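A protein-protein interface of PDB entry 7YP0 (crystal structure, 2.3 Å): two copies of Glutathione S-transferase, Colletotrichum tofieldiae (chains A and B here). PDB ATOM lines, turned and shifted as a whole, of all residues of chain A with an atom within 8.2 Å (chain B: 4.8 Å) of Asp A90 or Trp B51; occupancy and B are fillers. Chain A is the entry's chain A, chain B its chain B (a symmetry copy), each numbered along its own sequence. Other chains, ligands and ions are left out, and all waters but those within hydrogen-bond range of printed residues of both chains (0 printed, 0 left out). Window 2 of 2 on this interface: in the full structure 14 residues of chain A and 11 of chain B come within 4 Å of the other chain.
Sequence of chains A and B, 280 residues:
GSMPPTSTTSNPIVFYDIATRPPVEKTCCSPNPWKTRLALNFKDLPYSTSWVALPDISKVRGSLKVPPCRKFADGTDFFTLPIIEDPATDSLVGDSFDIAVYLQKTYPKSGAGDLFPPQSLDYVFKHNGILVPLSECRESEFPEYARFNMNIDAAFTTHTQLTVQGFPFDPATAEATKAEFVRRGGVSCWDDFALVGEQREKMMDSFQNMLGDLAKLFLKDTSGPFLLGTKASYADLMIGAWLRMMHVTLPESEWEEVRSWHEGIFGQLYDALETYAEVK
Of the 11 printed residues of chain A, 2 touch a printed residue of chain B. Printed residues of chain A that touch a printed residue of chain B: Glu A85 and Asp A90. Along chain A the printed residues that touch a printed residue of chain B span positions 85 to 90. Among the printed residues, 4 pairs touch across the chains. Among the printed residues, no Asp or Glu carboxylate lies within 4 Å of a Lys or Arg side-chain nitrogen of the other chain.
Among the printed residues, pairs that only touch across the chains: Asp A90 with Trp B51 (3.5 Å) and Asp A90 with Val B52 (3.5 Å).
The side-chain carboxylate of Glu A85 is in hydrogen-bond range of the side-chain hydroxyl of Ser B50 (3.4 Å). The backbone NH of Ala B53 is in hydrogen-bond range of the backbone carbonyl oxygen of Asp A90, at 2.9 Å.
Asp A90 touches just these residues of chain B: Trp B51, Val B52 and Ala B53. Trp B51 touches just one residue of chain A: Asp A90. Printed residues of chain A within 4 Å of Ser B50: Glu A85. Of the printed residues of chain A, Ala B53 touches Asp A90. Pro A87 touches none of the printed residues of chain B. The nearest printed residue of chain B that does not touch Asp A90 is Ala B19 (5.8 Å). The nearest printed residue of chain A that does not touch Ser B50 is Pro A87 (6.6 Å).
The backbone carbonyl oxygen (O) of Ser B50 sits at hydrogen-bond distance from the backbone NH (N) of Asp B17 (3.1 Å). The backbone carbonyl oxygen (O) of Asp B17 is in hydrogen-bond range of the backbone NH (N) of Val B52 (3.1 Å). O of Val B52 sits at hydrogen-bond distance from N of Ala B19.
No position is printed for both chains.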
ATOM      1  N   ILE A  84     -21.012   5.669 -12.403  1.00  0.00           N
ATOM      2  CA  ILE A  84     -21.554   5.538 -13.752  1.00  0.00           C
ATOM      3  C   ILE A  84     -20.849   6.503 -14.699  1.00  0.00           C
ATOM      4  O   ILE A  84     -20.414   7.592 -14.316  1.00  0.00           O
ATOM      5  CB  ILE A  84     -23.084   5.761 -13.807  1.00  0.00           C
ATOM      6  CG1 ILE A  84     -23.451   7.142 -13.277  1.00  0.00           C
ATOM      7  CG2 ILE A  84     -23.822   4.679 -13.045  1.00  0.00           C
ATOM      8  CD1 ILE A  84     -24.628   7.764 -13.998  1.00  0.00           C
ATOM      9  N   GLU A  85     -20.744   6.088 -15.954  1.00  0.00           N
ATOM     10  CA  GLU A  85     -20.387   6.969 -17.055  1.00  0.00           C
ATOM     11  C   GLU A  85     -21.617   7.138 -17.935  1.00  0.00           C
ATOM     12  O   GLU A  85     -22.175   6.148 -18.425  1.00  0.00           O
ATOM     13  CB  GLU A  85     -19.209   6.412 -17.859  1.00  0.00           C
ATOM     14  CG  GLU A  85     -18.824   7.216 -19.118  1.00  0.00           C
ATOM     15  CD  GLU A  85     -18.957   6.427 -20.444  1.00  0.00           C
ATOM     16  OE1 GLU A  85     -19.670   6.920 -21.345  1.00  0.00           O
ATOM     17  OE2 GLU A  85     -18.316   5.344 -20.616  1.00  0.00           O
ATOM     18  N   ASP A  86     -22.042   8.386 -18.123  1.00  0.00           N
ATOM     19  CA  ASP A  86     -23.169   8.706 -18.997  1.00  0.00           C
ATOM     20  C   ASP A  86     -22.668   9.403 -20.254  1.00  0.00           C
ATOM     21  O   ASP A  86     -22.445  10.625 -20.240  1.00  0.00           O
ATOM     22  CB  ASP A  86     -24.194   9.583 -18.276  1.00  0.00           C
ATOM     23  CG  ASP A  86     -25.499   9.721 -19.061  1.00  0.00           C
ATOM     24  OD1 ASP A  86     -25.575   9.219 -20.203  1.00  0.00           O
ATOM     25  OD2 ASP A  86     -26.454  10.322 -18.528  1.00  0.00           O
ATOM     26  N   PRO A  87     -22.498   8.679 -21.365  1.00  0.00           N
ATOM     27  CA  PRO A  87     -21.980   9.309 -22.591  1.00  0.00           C
ATOM     28  C   PRO A  87     -22.910  10.356 -23.183  1.00  0.00           C
ATOM     29  O   PRO A  87     -22.465  11.139 -24.033  1.00  0.00           O
ATOM     30  CB  PRO A  87     -21.792   8.125 -23.549  1.00  0.00           C
ATOM     31  CG  PRO A  87     -22.684   7.072 -23.044  1.00  0.00           C
ATOM     32  CD  PRO A  87     -22.858   7.266 -21.563  1.00  0.00           C
ATOM     33  N   ALA A  88     -24.174  10.405 -22.758  1.00  0.00           N
ATOM     34  CA  ALA A  88     -25.071  11.453 -23.220  1.00  0.00           C
ATOM     35  C   ALA A  88     -24.627  12.828 -22.750  1.00  0.00           C
ATOM     36  O   ALA A  88     -24.990  13.829 -23.380  1.00  0.00           O
ATOM     37  CB  ALA A  88     -26.502  11.180 -22.749  1.00  0.00           C
ATOM     38  N   THR A  89     -23.862  12.904 -21.652  1.00  0.00           N
ATOM     39  CA  THR A  89     -23.341  14.171 -21.154  1.00  0.00           C
ATOM     40  C   THR A  89     -21.843  14.127 -20.866  1.00  0.00           C
ATOM     41  O   THR A  89     -21.332  15.044 -20.203  1.00  0.00           O
ATOM     42  CB  THR A  89     -24.081  14.610 -19.883  1.00  0.00           C
ATOM     43  OG1 THR A  89     -23.852  13.648 -18.844  1.00  0.00           O
ATOM     44  CG2 THR A  89     -25.575  14.743 -20.145  1.00  0.00           C
ATOM     45  N   ASP A  90     -21.135  13.094 -21.335  1.00  0.00           N
ATOM     46  CA  ASP A  90     -19.704  12.894 -21.067  1.00  0.00           C
ATOM     47  C   ASP A  90     -19.353  13.143 -19.597  1.00  0.00           C
ATOM     48  O   ASP A  90     -18.374  13.824 -19.268  1.00  0.00           O
ATOM     49  CB  ASP A  90     -18.850  13.768 -21.982  1.00  0.00           C
ATOM     50  CG  ASP A  90     -19.349  13.773 -23.417  1.00  0.00           C
ATOM     51  OD1 ASP A  90     -19.651  14.868 -23.944  1.00  0.00           O
ATOM     52  OD2 ASP A  90     -19.424  12.682 -24.026  1.00  0.00           O
ATOM     53  N   SER A  91     -20.171  12.583 -18.704  1.00  0.00           N
ATOM     54  CA  SER A  91     -19.989  12.755 -17.273  1.00  0.00           C
ATOM     55  C   SER A  91     -19.592  11.441 -16.620  1.00  0.00           C
ATOM     56  O   SER A  91     -19.982  10.359 -17.059  1.00  0.00           O
ATOM     57  CB  SER A  91     -21.247  13.281 -16.591  1.00  0.00           C
ATOM     58  OG  SER A  91     -21.909  14.230 -17.396  1.00  0.00           O
ATOM     59  N   LEU A  92     -18.821  11.568 -15.551  1.00  0.00           N
ATOM     60  CA  LEU A  92     -18.401  10.460 -14.713  1.00  0.00           C
ATOM     61  C   LEU A  92     -18.825  10.830 -13.306  1.00  0.00           C
ATOM     62  O   LEU A  92     -18.356  11.840 -12.773  1.00  0.00           O
ATOM     63  CB  LEU A  92     -16.883  10.262 -14.801  1.00  0.00           C
ATOM     64  CG  LEU A  92     -16.271   8.883 -14.611  1.00  0.00           C
ATOM     65  CD1 LEU A  92     -16.923   7.885 -15.548  1.00  0.00           C
ATOM     66  CD2 LEU A  92     -14.774   8.955 -14.879  1.00  0.00           C
ATOM     67  N   VAL A  93     -19.735  10.046 -12.718  1.00  0.00           N
ATOM     68  CA  VAL A  93     -20.368  10.388 -11.446  1.00  0.00           C
ATOM     69  C   VAL A  93     -20.207   9.228 -10.471  1.00  0.00           C
ATOM     70  O   VAL A  93     -20.598   8.093 -10.772  1.00  0.00           O
ATOM     71  CB  VAL A  93     -21.865  10.733 -11.621  1.00  0.00           C
ATOM     72  CG1 VAL A  93     -22.432  11.341 -10.331  1.00  0.00           C
ATOM     73  CG2 VAL A  93     -22.068  11.686 -12.793  1.00  0.00           C
ATOM     74  N   TYR A 102     -28.156  13.129  -9.929  1.00  0.00           N
ATOM     75  CA  TYR A 102     -27.826  13.349 -11.332  1.00  0.00           C
ATOM     76  C   TYR A 102     -28.888  12.763 -12.267  1.00  0.00           C
ATOM     77  O   TYR A 102     -29.230  13.378 -13.281  1.00  0.00           O
ATOM     78  CB  TYR A 102     -26.451  12.761 -11.650  1.00  0.00           C
ATOM     79  CG  TYR A 102     -26.179  12.663 -13.146  1.00  0.00           C
ATOM     80  CD1 TYR A 102     -26.532  11.525 -13.861  1.00  0.00           C
ATOM     81  CD2 TYR A 102     -25.589  13.721 -13.846  1.00  0.00           C
ATOM     82  CE1 TYR A 102     -26.310  11.432 -15.217  1.00  0.00           C
ATOM     83  CE2 TYR A 102     -25.343  13.622 -15.218  1.00  0.00           C
ATOM     84  CZ  TYR A 102     -25.720  12.471 -15.893  1.00  0.00           C
ATOM     85  OH  TYR A 102     -25.515  12.333 -17.254  1.00  0.00           O
ATOM     86  N   ASP B  17     -10.378   9.365 -20.933  1.00  0.00           N
ATOM     87  CA  ASP B  17      -9.461  10.428 -21.318  1.00  0.00           C
ATOM     88  C   ASP B  17     -10.165  11.781 -21.170  1.00  0.00           C
ATOM     89  O   ASP B  17     -11.392  11.855 -21.082  1.00  0.00           O
ATOM     90  CB  ASP B  17      -8.999  10.198 -22.773  1.00  0.00           C
ATOM     91  CG  ASP B  17      -7.641  10.828 -23.107  1.00  0.00           C
ATOM     92  OD1 ASP B  17      -7.171  11.786 -22.435  1.00  0.00           O
ATOM     93  OD2 ASP B  17      -7.057  10.367 -24.113  1.00  0.00           O
ATOM     94  N   ILE B  18      -9.380  12.856 -21.170  1.00  0.00           N
ATOM     95  CA  ILE B  18      -9.873  14.200 -20.884  1.00  0.00           C
ATOM     96  C   ILE B  18     -10.303  14.867 -22.188  1.00  0.00           C
ATOM     97  O   ILE B  18      -9.486  15.077 -23.097  1.00  0.00           O
ATOM     98  CB  ILE B  18      -8.801  15.033 -20.163  1.00  0.00           C
ATOM     99  CG1 ILE B  18      -8.468  14.409 -18.801  1.00  0.00           C
ATOM    100  CG2 ILE B  18      -9.241  16.483 -20.020  1.00  0.00           C
ATOM    101  CD1 ILE B  18      -7.203  14.970 -18.155  1.00  0.00           C
ATOM    102  N   ALA B  19     -11.588  15.191 -22.280  1.00  0.00           N
ATOM    103  CA  ALA B  19     -12.141  15.805 -23.480  1.00  0.00           C
ATOM    104  C   ALA B  19     -11.555  17.202 -23.676  1.00  0.00           C
ATOM    105  O   ALA B  19     -11.575  18.033 -22.764  1.00  0.00           O
ATOM    106  CB  ALA B  19     -13.673  15.874 -23.382  1.00  0.00           C
ATOM    107  N   VAL B  24     -11.123  15.940 -31.312  1.00  0.00           N
ATOM    108  CA  VAL B  24     -10.462  15.480 -30.090  1.00  0.00           C
ATOM    109  C   VAL B  24      -9.252  14.603 -30.396  1.00  0.00           C
ATOM    110  O   VAL B  24      -8.255  14.649 -29.670  1.00  0.00           O
ATOM    111  CB  VAL B  24     -11.482  14.775 -29.173  1.00  0.00           C
ATOM    112  CG1 VAL B  24     -11.590  13.287 -29.499  1.00  0.00           C
ATOM    113  CG2 VAL B  24     -11.115  14.983 -27.710  1.00  0.00           C
ATOM    114  N   CYS B  28      -6.187  16.349 -28.082  1.00  0.00           N
ATOM    115  CA  CYS B  28      -5.971  15.770 -26.758  1.00  0.00           C
ATOM    116  C   CYS B  28      -4.507  15.916 -26.357  1.00  0.00           C
ATOM    117  O   CYS B  28      -3.596  15.596 -27.125  1.00  0.00           O
ATOM    118  CB  CYS B  28      -6.414  14.303 -26.704  1.00  0.00           C
ATOM    119  SG  CYS B  28      -5.660  13.173 -27.887  1.00  0.00           S
ATOM    120  N   ARG B  37      -2.109   6.101 -22.902  1.00  0.00           N
ATOM    121  CA  ARG B  37      -2.340   5.806 -24.316  1.00  0.00           C
ATOM    122  C   ARG B  37      -1.097   5.219 -24.979  1.00  0.00           C
ATOM    123  O   ARG B  37      -1.176   4.233 -25.723  1.00  0.00           O
ATOM    124  CB  ARG B  37      -2.775   7.081 -25.044  1.00  0.00           C
ATOM    125  CG  ARG B  37      -3.103   6.867 -26.526  1.00  0.00           C
ATOM    126  CD  ARG B  37      -3.671   8.143 -27.152  1.00  0.00           C
ATOM    127  NE  ARG B  37      -4.931   8.552 -26.539  1.00  0.00           N
ATOM    128  CZ  ARG B  37      -6.098   7.969 -26.781  1.00  0.00           C
ATOM    129  NH1 ARG B  37      -6.202   6.954 -27.626  1.00  0.00           N
ATOM    130  NH2 ARG B  37      -7.191   8.423 -26.173  1.00  0.00           N
ATOM    131  N   THR B  49     -11.829   4.629 -26.328  1.00  0.00           N
ATOM    132  CA  THR B  49     -11.701   5.795 -25.470  1.00  0.00           C
ATOM    133  C   THR B  49     -13.066   6.410 -25.210  1.00  0.00           C
ATOM    134  O   THR B  49     -13.844   6.634 -26.143  1.00  0.00           O
ATOM    135  CB  THR B  49     -10.779   6.839 -26.097  1.00  0.00           C
ATOM    136  OG1 THR B  49      -9.513   6.235 -26.378  1.00  0.00           O
ATOM    137  CG2 THR B  49     -10.575   8.013 -25.137  1.00  0.00           C
ATOM    138  N   SER B  50     -13.341   6.696 -23.944  1.00  0.00           N
ATOM    139  CA  SER B  50     -14.462   7.532 -23.547  1.00  0.00           C
ATOM    140  C   SER B  50     -13.890   8.879 -23.145  1.00  0.00           C
ATOM    141  O   SER B  50     -13.181   8.980 -22.138  1.00  0.00           O
ATOM    142  CB  SER B  50     -15.233   6.899 -22.394  1.00  0.00           C
ATOM    143  OG  SER B  50     -15.724   5.624 -22.768  1.00  0.00           O
ATOM    144  N   TRP B  51     -14.175   9.901 -23.941  1.00  0.00           N
ATOM    145  CA  TRP B  51     -13.777  11.267 -23.626  1.00  0.00           C
ATOM    146  C   TRP B  51     -14.811  11.879 -22.705  1.00  0.00           C
ATOM    147  O   TRP B  51     -15.951  12.118 -23.118  1.00  0.00           O
ATOM    148  CB  TRP B  51     -13.663  12.098 -24.894  1.00  0.00           C
ATOM    149  CG  TRP B  51     -12.851  11.450 -25.917  1.00  0.00           C
ATOM    150  CD1 TRP B  51     -13.279  10.603 -26.910  1.00  0.00           C
ATOM    151  CD2 TRP B  51     -11.452  11.585 -26.076  1.00  0.00           C
ATOM    152  NE1 TRP B  51     -12.214  10.203 -27.676  1.00  0.00           N
ATOM    153  CE2 TRP B  51     -11.078  10.794 -27.182  1.00  0.00           C
ATOM    154  CE3 TRP B  51     -10.470  12.292 -25.384  1.00  0.00           C
ATOM    155  CZ2 TRP B  51      -9.771  10.710 -27.618  1.00  0.00           C
ATOM    156  CZ3 TRP B  51      -9.181  12.196 -25.812  1.00  0.00           C
ATOM    157  CH2 TRP B  51      -8.839  11.419 -26.919  1.00  0.00           C
ATOM    158  N   VAL B  52     -14.414  12.181 -21.483  1.00  0.00           N
ATOM    159  CA  VAL B  52     -15.336  12.763 -20.526  1.00  0.00           C
ATOM    160  C   VAL B  52     -14.805  14.111 -20.060  1.00  0.00           C
ATOM    161  O   VAL B  52     -13.597  14.380 -20.082  1.00  0.00           O
ATOM    162  CB  VAL B  52     -15.566  11.817 -19.332  1.00  0.00           C
ATOM    163  CG1 VAL B  52     -16.176  10.511 -19.820  1.00  0.00           C
ATOM    164  CG2 VAL B  52     -14.271  11.571 -18.626  1.00  0.00           C
ATOM    165  N   ALA B  53     -15.730  14.975 -19.655  1.00  0.00           N
ATOM    166  CA  ALA B  53     -15.338  16.199 -18.993  1.00  0.00           C
ATOM    167  C   ALA B  53     -14.584  15.847 -17.715  1.00  0.00           C
ATOM    168  O   ALA B  53     -14.800  14.794 -17.102  1.00  0.00           O
ATOM    169  CB  ALA B  53     -16.566  17.051 -18.686  1.00  0.00           C
ATOM    170  N   VAL B 279      -4.565   7.610 -31.853  1.00  0.00           N
ATOM    171  CA  VAL B 279      -5.657   8.028 -30.972  1.00  0.00           C
ATOM    172  C   VAL B 279      -6.881   7.210 -31.384  1.00  0.00           C
ATOM    173  O   VAL B 279      -7.624   7.570 -32.303  1.00  0.00           O
ATOM    174  CB  VAL B 279      -5.904   9.533 -31.046  1.00  0.00           C
ATOM    175  CG1 VAL B 279      -7.048   9.916 -30.141  1.00  0.00           C
ATOM    176  CG2 VAL B 279      -4.637  10.304 -30.668  1.00  0.00           C
